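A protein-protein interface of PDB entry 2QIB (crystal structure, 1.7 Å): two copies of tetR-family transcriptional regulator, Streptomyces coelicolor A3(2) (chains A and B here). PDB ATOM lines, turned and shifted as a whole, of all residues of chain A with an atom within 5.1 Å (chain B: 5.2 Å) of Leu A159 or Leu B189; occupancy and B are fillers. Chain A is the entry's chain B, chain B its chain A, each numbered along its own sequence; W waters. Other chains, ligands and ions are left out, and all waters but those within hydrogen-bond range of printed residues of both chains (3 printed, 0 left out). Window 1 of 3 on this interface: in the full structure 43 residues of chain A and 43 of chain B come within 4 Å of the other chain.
The backbone carbonyl oxygen (O) of Val B152 is in hydrogen-bond range of the side-chain hydroxyl (OG) of Ser B155.
O of Leu A159 lies within hydrogen-bond range of OG1 of Thr A163 (2.8 Å).
Among the printed residues, pairs that only touch across the chains: Asp A185 with Leu B189 (3.3 Å), Leu A189 with Asp B185 (3.4 Å), Asp A185 with Val B192 (3.4 Å), Ser A162 with Ser B155 (3.5 Å), Ser A155 with Leu B159 (3.6 Å), Leu A159 with Ser B155 (3.6 Å), Leu A189 with Leu B159 (3.8 Å) and Leu A159 with Leu B189 (3.9 Å).
Leu A159 touches two residues of chain B.
Leu B189 touches two residues of chain A.
Printed residues of chain B within 4 Å of Ser A162: Ser B155.
Printed residues of chain A within 4 Å of Asp B185: Leu A189.
Of the printed residues of chain B, Leu A189 touches Leu B159 and Asp B185.
Of the printed residues of chain A, Val B192 touches Asp A185.
Of the printed residues of chain A, Leu B159 touches Ser A155 (3.6 Å) and Leu A189 (3.8 Å).
Phe B186 touches none of the printed residues of chain A.
Val B152 touches none of the printed residues of chain A.
The nearest residue of chain B that does not touch Leu A159 is Leu B159 (4.5 Å).
The nearest printed residue of chain A that does not touch Val B192 is Leu A182 (5.7 Å).
Of the 13 printed residues of chain A, 5 touch a printed residue of chain B.
Hydrophobic or aromatic side chains of chain A within 4 Å of the printed part of chain B: Leu A159 and Leu A189.
Of the 14 printed residues of chain B, 5 touch a printed residue of chain A.
Ser A155 touches Leu B159, and with the chains exchanged Leu A159 touches Ser B155.
Leu A159 touches Leu B189, and with the chains exchanged Leu A189 touches Leu B159.
Asp A185 touches Leu B189, and with the chains exchanged Leu A189 touches Asp B185.
5 positions are printed for both chains.
Of the 8 pairs that touch across the chains among the printed residues, 6 have their exchanged pair printed and touching as well.
Water W1 bridges OD1 of Asp A185 (2.6 Å) and O of Leu B189 (2.8 Å).
Water W2 lies within hydrogen-bond range of the side-chain carboxylate of Asp B185 (2.7 Å) and the backbone carbonyl oxygen of Leu A189 (2.9 Å).
Water W3 lies within hydrogen-bond range of the backbone NH (N) of Leu A159 (2.9 Å), the backbone NH (N) of Leu B159 (2.9 Å) and the backbone carbonyl oxygen (O) of Ser A158 (3.4 Å).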
ATOM      1  N   SER A 155      23.449  -0.775 -33.021  1.00  0.00           N
ATOM      2  CA  SER A 155      24.360   0.018 -32.190  1.00  0.00           C
ATOM      3  C   SER A 155      23.536   0.674 -31.081  1.00  0.00           C
ATOM      4  O   SER A 155      23.987   0.758 -29.932  1.00  0.00           O
ATOM      5  CB  SER A 155      25.138   1.059 -32.995  1.00  0.00           C
ATOM      6  OG  SER A 155      24.308   2.102 -33.407  1.00  0.00           O
ATOM      7  N   TRP A 156      22.304   1.043 -31.399  1.00  0.00           N
ATOM      8  CA  TRP A 156      21.421   1.611 -30.350  1.00  0.00           C
ATOM      9  C   TRP A 156      21.063   0.565 -29.286  1.00  0.00           C
ATOM     10  O   TRP A 156      21.038   0.851 -28.086  1.00  0.00           O
ATOM     11  CB  TRP A 156      20.155   2.243 -30.939  1.00  0.00           C
ATOM     12  CG  TRP A 156      19.291   2.777 -29.884  1.00  0.00           C
ATOM     13  CD1 TRP A 156      19.339   4.028 -29.302  1.00  0.00           C
ATOM     14  CD2 TRP A 156      18.262   2.049 -29.198  1.00  0.00           C
ATOM     15  NE1 TRP A 156      18.345   4.125 -28.326  1.00  0.00           N
ATOM     16  CE2 TRP A 156      17.700   2.916 -28.231  1.00  0.00           C
ATOM     17  CE3 TRP A 156      17.763   0.744 -29.319  1.00  0.00           C
ATOM     18  CZ2 TRP A 156      16.644   2.513 -27.390  1.00  0.00           C
ATOM     19  CZ3 TRP A 156      16.692   0.333 -28.471  1.00  0.00           C
ATOM     20  CH2 TRP A 156      16.153   1.229 -27.535  1.00  0.00           C
ATOM     21  N   ILE A 157      20.802  -0.650 -29.731  1.00  0.00           N
ATOM     22  CA  ILE A 157      20.524  -1.753 -28.788  1.00  0.00           C
ATOM     23  C   ILE A 157      21.717  -1.884 -27.820  1.00  0.00           C
ATOM     24  O   ILE A 157      21.536  -1.972 -26.615  1.00  0.00           O
ATOM     25  CB  ILE A 157      20.218  -3.054 -29.536  1.00  0.00           C
ATOM     26  CG1 ILE A 157      18.814  -2.977 -30.208  1.00  0.00           C
ATOM     27  CG2 ILE A 157      20.200  -4.258 -28.595  1.00  0.00           C
ATOM     28  CD1 ILE A 157      18.619  -4.022 -31.337  1.00  0.00           C
ATOM     29  N   SER A 158      22.937  -1.829 -28.346  1.00  0.00           N
ATOM     30  CA  SER A 158      24.124  -1.879 -27.473  1.00  0.00           C
ATOM     31  C   SER A 158      24.158  -0.694 -26.499  1.00  0.00           C
ATOM     32  O   SER A 158      24.535  -0.860 -25.337  1.00  0.00           O
ATOM     33  CB  SER A 158      25.433  -1.925 -28.272  1.00  0.00           C
ATOM     34  OG  SER A 158      25.443  -3.053 -29.153  1.00  0.00           O
ATOM     35  N   LEU A 159      23.806   0.499 -27.011  1.00  0.00           N
ATOM     36  CA  LEU A 159      23.743   1.719 -26.209  1.00  0.00           C
ATOM     37  C   LEU A 159      22.721   1.544 -25.051  1.00  0.00           C
ATOM     38  O   LEU A 159      22.974   1.943 -23.899  1.00  0.00           O
ATOM     39  CB  LEU A 159      23.315   2.898 -27.095  1.00  0.00           C
ATOM     40  CG  LEU A 159      23.337   4.259 -26.366  1.00  0.00           C
ATOM     41  CD1 LEU A 159      24.769   4.674 -26.153  1.00  0.00           C
ATOM     42  CD2 LEU A 159      22.684   5.293 -27.225  1.00  0.00           C
ATOM     43  N   ALA A 160      21.565   0.983 -25.385  1.00  0.00           N
ATOM     44  CA  ALA A 160      20.508   0.756 -24.390  1.00  0.00           C
ATOM     45  C   ALA A 160      20.958  -0.269 -23.308  1.00  0.00           C
ATOM     46  O   ALA A 160      20.712  -0.078 -22.106  1.00  0.00           O
ATOM     47  CB  ALA A 160      19.249   0.297 -25.080  1.00  0.00           C
ATOM     48  N   GLU A 161      21.618  -1.352 -23.729  1.00  0.00           N
ATOM     49  CA  GLU A 161      22.197  -2.329 -22.790  1.00  0.00           C
ATOM     50  C   GLU A 161      23.204  -1.617 -21.870  1.00  0.00           C
ATOM     51  O   GLU A 161      23.155  -1.738 -20.637  1.00  0.00           O
ATOM     52  CB  GLU A 161      22.899  -3.369 -23.669  1.00  0.00           C
ATOM     53  CG  GLU A 161      23.414  -4.593 -23.034  1.00  0.00           C
ATOM     54  CD  GLU A 161      24.007  -5.521 -24.109  1.00  0.00           C
ATOM     55  OE1 GLU A 161      23.376  -5.680 -25.185  1.00  0.00           O
ATOM     56  OE2 GLU A 161      25.110  -6.040 -23.866  1.00  0.00           O
ATOM     57  N   SER A 162      24.125  -0.857 -22.472  1.00  0.00           N
ATOM     58  CA  SER A 162      25.150  -0.158 -21.693  1.00  0.00           C
ATOM     59  C   SER A 162      24.555   0.808 -20.670  1.00  0.00           C
ATOM     60  O   SER A 162      24.977   0.862 -19.502  1.00  0.00           O
ATOM     61  CB  SER A 162      26.094   0.575 -22.632  1.00  0.00           C
ATOM     62  OG  SER A 162      27.129   1.237 -21.877  1.00  0.00           O
ATOM     63  N   THR A 163      23.562   1.554 -21.118  1.00  0.00           N
ATOM     64  CA  THR A 163      22.918   2.597 -20.327  1.00  0.00           C
ATOM     65  C   THR A 163      22.252   1.945 -19.111  1.00  0.00           C
ATOM     66  O   THR A 163      22.420   2.427 -17.991  1.00  0.00           O
ATOM     67  CB  THR A 163      21.918   3.330 -21.179  1.00  0.00           C
ATOM     68  OG1 THR A 163      22.642   4.131 -22.132  1.00  0.00           O
ATOM     69  CG2 THR A 163      21.041   4.269 -20.301  1.00  0.00           C
ATOM     70  N   ALA A 164      21.547   0.835 -19.330  1.00  0.00           N
ATOM     71  CA  ALA A 164      20.862   0.139 -18.222  1.00  0.00           C
ATOM     72  C   ALA A 164      21.901  -0.391 -17.205  1.00  0.00           C
ATOM     73  O   ALA A 164      21.718  -0.289 -15.991  1.00  0.00           O
ATOM     74  CB  ALA A 164      20.007  -1.040 -18.783  1.00  0.00           C
ATOM     75  N   LEU A 182      17.218   7.604 -23.774  1.00  0.00           N
ATOM     76  CA  LEU A 182      17.385   6.541 -24.777  1.00  0.00           C
ATOM     77  C   LEU A 182      16.514   6.721 -26.030  1.00  0.00           C
ATOM     78  O   LEU A 182      16.949   6.410 -27.165  1.00  0.00           O
ATOM     79  CB  LEU A 182      17.181   5.155 -24.160  1.00  0.00           C
ATOM     80  CG  LEU A 182      18.401   4.729 -23.338  1.00  0.00           C
ATOM     81  CD1 LEU A 182      18.040   3.491 -22.481  1.00  0.00           C
ATOM     82  CD2 LEU A 182      19.659   4.474 -24.212  1.00  0.00           C
ATOM     83  N   ASP A 185      18.215   9.406 -27.897  1.00  0.00           N
ATOM     84  CA  ASP A 185      19.446   8.823 -28.448  1.00  0.00           C
ATOM     85  C   ASP A 185      19.144   8.045 -29.727  1.00  0.00           C
ATOM     86  O   ASP A 185      19.921   8.093 -30.649  1.00  0.00           O
ATOM     87  CB  ASP A 185      20.094   7.860 -27.431  1.00  0.00           C
ATOM     88  CG  ASP A 185      20.733   8.561 -26.241  1.00  0.00           C
ATOM     89  OD1 ASP A 185      20.994   9.798 -26.276  1.00  0.00           O
ATOM     90  OD2 ASP A 185      20.988   7.833 -25.262  1.00  0.00           O
ATOM     91  N   LEU A 189      21.042   8.966 -33.127  1.00  0.00           N
ATOM     92  CA  LEU A 189      21.871   8.054 -33.925  1.00  0.00           C
ATOM     93  C   LEU A 189      21.336   7.974 -35.369  1.00  0.00           C
ATOM     94  O   LEU A 189      22.108   8.033 -36.333  1.00  0.00           O
ATOM     95  CB  LEU A 189      21.971   6.678 -33.287  1.00  0.00           C
ATOM     96  CG  LEU A 189      22.668   6.708 -31.893  1.00  0.00           C
ATOM     97  CD1 LEU A 189      22.569   5.298 -31.278  1.00  0.00           C
ATOM     98  CD2 LEU A 189      24.157   7.198 -31.982  1.00  0.00           C
ATOM     99  N   VAL B 152      27.398   9.024 -20.171  1.00  0.00           N
ATOM    100  CA  VAL B 152      27.496   9.374 -21.594  1.00  0.00           C
ATOM    101  C   VAL B 152      28.810   8.848 -22.153  1.00  0.00           C
ATOM    102  O   VAL B 152      28.823   8.221 -23.225  1.00  0.00           O
ATOM    103  CB  VAL B 152      27.364  10.879 -21.853  1.00  0.00           C
ATOM    104  CG1 VAL B 152      27.729  11.187 -23.314  1.00  0.00           C
ATOM    105  CG2 VAL B 152      25.944  11.313 -21.536  1.00  0.00           C
ATOM    106  N   SER B 155      28.963   4.962 -22.165  1.00  0.00           N
ATOM    107  CA  SER B 155      27.983   4.401 -23.113  1.00  0.00           C
ATOM    108  C   SER B 155      28.458   4.680 -24.559  1.00  0.00           C
ATOM    109  O   SER B 155      28.236   3.829 -25.458  1.00  0.00           O
ATOM    110  CB  SER B 155      26.558   4.935 -22.882  1.00  0.00           C
ATOM    111  OG  SER B 155      26.493   6.308 -23.162  1.00  0.00           O
ATOM    112  N   TRP B 156      29.174   5.791 -24.757  1.00  0.00           N
ATOM    113  CA  TRP B 156      29.762   6.077 -26.078  1.00  0.00           C
ATOM    114  C   TRP B 156      30.859   5.066 -26.411  1.00  0.00           C
ATOM    115  O   TRP B 156      30.951   4.603 -27.538  1.00  0.00           O
ATOM    116  CB  TRP B 156      30.320   7.483 -26.185  1.00  0.00           C
ATOM    117  CG  TRP B 156      30.876   7.739 -27.562  1.00  0.00           C
ATOM    118  CD1 TRP B 156      30.209   8.171 -28.688  1.00  0.00           C
ATOM    119  CD2 TRP B 156      32.230   7.520 -27.954  1.00  0.00           C
ATOM    120  NE1 TRP B 156      31.116   8.266 -29.768  1.00  0.00           N
ATOM    121  CE2 TRP B 156      32.339   7.845 -29.333  1.00  0.00           C
ATOM    122  CE3 TRP B 156      33.374   7.054 -27.272  1.00  0.00           C
ATOM    123  CZ2 TRP B 156      33.558   7.751 -30.023  1.00  0.00           C
ATOM    124  CZ3 TRP B 156      34.602   6.978 -27.983  1.00  0.00           C
ATOM    125  CH2 TRP B 156      34.656   7.305 -29.339  1.00  0.00           C
ATOM    126  N   LEU B 159      29.193   2.147 -27.629  1.00  0.00           N
ATOM    127  CA  LEU B 159      28.705   2.466 -28.973  1.00  0.00           C
ATOM    128  C   LEU B 159      29.853   2.288 -30.003  1.00  0.00           C
ATOM    129  O   LEU B 159      29.646   1.749 -31.120  1.00  0.00           O
ATOM    130  CB  LEU B 159      28.199   3.929 -29.025  1.00  0.00           C
ATOM    131  CG  LEU B 159      27.582   4.276 -30.379  1.00  0.00           C
ATOM    132  CD1 LEU B 159      26.233   3.537 -30.516  1.00  0.00           C
ATOM    133  CD2 LEU B 159      27.361   5.776 -30.415  1.00  0.00           C
ATOM    134  N   HIS B 184      30.380  12.542 -34.525  1.00  0.00           N
ATOM    135  CA  HIS B 184      29.080  13.195 -34.416  1.00  0.00           C
ATOM    136  C   HIS B 184      28.201  12.560 -33.336  1.00  0.00           C
ATOM    137  O   HIS B 184      27.529  13.277 -32.601  1.00  0.00           O
ATOM    138  CB  HIS B 184      28.354  13.112 -35.732  1.00  0.00           C
ATOM    139  CG  HIS B 184      28.954  13.978 -36.797  1.00  0.00           C
ATOM    140  ND1 HIS B 184      29.454  15.243 -36.535  1.00  0.00           N
ATOM    141  CD2 HIS B 184      29.076  13.790 -38.133  1.00  0.00           C
ATOM    142  CE1 HIS B 184      29.859  15.790 -37.670  1.00  0.00           C
ATOM    143  NE2 HIS B 184      29.662  14.922 -38.651  1.00  0.00           N
ATOM    144  N   ASP B 185      28.229  11.228 -33.238  1.00  0.00           N
ATOM    145  CA  ASP B 185      27.463  10.507 -32.201  1.00  0.00           C
ATOM    146  C   ASP B 185      27.838  10.994 -30.805  1.00  0.00           C
ATOM    147  O   ASP B 185      26.978  11.149 -29.973  1.00  0.00           O
ATOM    148  CB  ASP B 185      27.734   9.015 -32.260  1.00  0.00           C
ATOM    149  CG  ASP B 185      27.079   8.342 -33.478  1.00  0.00           C
ATOM    150  OD1 ASP B 185      26.157   8.946 -34.068  1.00  0.00           O
ATOM    151  OD2 ASP B 185      27.488   7.184 -33.814  1.00  0.00           O
ATOM    152  N   PHE B 186      29.121  11.239 -30.568  1.00  0.00           N
ATOM    153  CA  PHE B 186      29.578  11.683 -29.257  1.00  0.00           C
ATOM    154  C   PHE B 186      28.920  13.040 -28.947  1.00  0.00           C
ATOM    155  O   PHE B 186      28.363  13.232 -27.877  1.00  0.00           O
ATOM    156  CB  PHE B 186      31.131  11.789 -29.242  1.00  0.00           C
ATOM    157  CG  PHE B 186      31.717  11.982 -27.839  1.00  0.00           C
ATOM    158  CD1 PHE B 186      32.317  10.928 -27.166  1.00  0.00           C
ATOM    159  CD2 PHE B 186      31.699  13.252 -27.247  1.00  0.00           C
ATOM    160  CE1 PHE B 186      32.842  11.091 -25.847  1.00  0.00           C
ATOM    161  CE2 PHE B 186      32.220  13.452 -25.952  1.00  0.00           C
ATOM    162  CZ  PHE B 186      32.794  12.367 -25.254  1.00  0.00           C
ATOM    163  N   ALA B 187      29.027  13.998 -29.879  1.00  0.00           N
ATOM    164  CA  ALA B 187      28.394  15.334 -29.692  1.00  0.00           C
ATOM    165  C   ALA B 187      26.889  15.177 -29.422  1.00  0.00           C
ATOM    166  O   ALA B 187      26.305  15.802 -28.499  1.00  0.00           O
ATOM    167  CB  ALA B 187      28.639  16.185 -30.941  1.00  0.00           C
ATOM    168  N   ALA B 188      26.250  14.334 -30.225  1.00  0.00           N
ATOM    169  CA  ALA B 188      24.800  14.181 -30.112  1.00  0.00           C
ATOM    170  C   ALA B 188      24.358  13.542 -28.791  1.00  0.00           C
ATOM    171  O   ALA B 188      23.403  14.025 -28.175  1.00  0.00           O
ATOM    172  CB  ALA B 188      24.232  13.431 -31.332  1.00  0.00           C
ATOM    173  N   LEU B 189      25.059  12.502 -28.355  1.00  0.00           N
ATOM    174  CA  LEU B 189      24.784  11.876 -27.044  1.00  0.00           C
ATOM    175  C   LEU B 189      24.960  12.889 -25.918  1.00  0.00           C
ATOM    176  O   LEU B 189      24.138  12.955 -25.021  1.00  0.00           O
ATOM    177  CB  LEU B 189      25.642  10.632 -26.792  1.00  0.00           C
ATOM    178  CG  LEU B 189      25.344   9.499 -27.784  1.00  0.00           C
ATOM    179  CD1 LEU B 189      26.318   8.357 -27.596  1.00  0.00           C
ATOM    180  CD2 LEU B 189      23.884   8.989 -27.698  1.00  0.00           C
ATOM    181  N   MET B 190      26.019  13.696 -25.985  1.00  0.00           N
ATOM    182  CA  MET B 190      26.221  14.712 -24.965  1.00  0.00           C
ATOM    183  C   MET B 190      25.113  15.755 -25.023  1.00  0.00           C
ATOM    184  O   MET B 190      24.610  16.191 -23.987  1.00  0.00           O
ATOM    185  CB  MET B 190      27.577  15.385 -25.145  1.00  0.00           C
ATOM    186  CG  MET B 190      28.698  14.377 -25.127  1.00  0.00           C
ATOM    187  SD  MET B 190      29.465  14.296 -23.350  1.00  0.00           S
ATOM    188  CE  MET B 190      30.354  16.069 -23.669  1.00  0.00           C
ATOM    189  N   ALA B 191      24.739  16.186 -26.224  1.00  0.00           N
ATOM    190  CA  ALA B 191      23.663  17.174 -26.358  1.00  0.00           C
ATOM    191  C   ALA B 191      22.314  16.682 -25.816  1.00  0.00           C
ATOM    192  O   ALA B 191      21.547  17.464 -25.240  1.00  0.00           O
ATOM    193  CB  ALA B 191      23.504  17.598 -27.776  1.00  0.00           C
ATOM    194  N   VAL B 192      22.016  15.409 -26.024  1.00  0.00           N
ATOM    195  CA  VAL B 192      20.776  14.829 -25.510  1.00  0.00           C
ATOM    196  C   VAL B 192      20.763  14.923 -23.981  1.00  0.00           C
ATOM    197  O   VAL B 192      19.774  15.367 -23.390  1.00  0.00           O
ATOM    198  CB  VAL B 192      20.565  13.365 -25.998  1.00  0.00           C
ATOM    199  CG1 VAL B 192      19.449  12.687 -25.229  1.00  0.00           C
ATOM    200  CG2 VAL B 192      20.233  13.376 -27.493  1.00  0.00           C
ATOM    201  N   SER B 193      21.872  14.545 -23.353  1.00  0.00           N
ATOM    202  CA  SER B 193      21.975  14.584 -21.895  1.00  0.00           C
ATOM    203  C   SER B 193      21.879  16.022 -21.376  1.00  0.00           C
ATOM    204  O   SER B 193      21.274  16.269 -20.347  1.00  0.00           O
ATOM    205  CB  SER B 193      23.278  13.971 -21.425  1.00  0.00           C
ATOM    206  OG  SER B 193      23.375  13.990 -20.006  1.00  0.00           O
HETATM  207  O   HOH W   1      22.629  10.682 -24.459  1.00  0.00           O
HETATM  208  O   HOH W   2      24.822   7.336 -35.737  1.00  0.00           O
HETATM  209  O   HOH W   3      26.612   0.916 -27.352  1.00  0.00           O
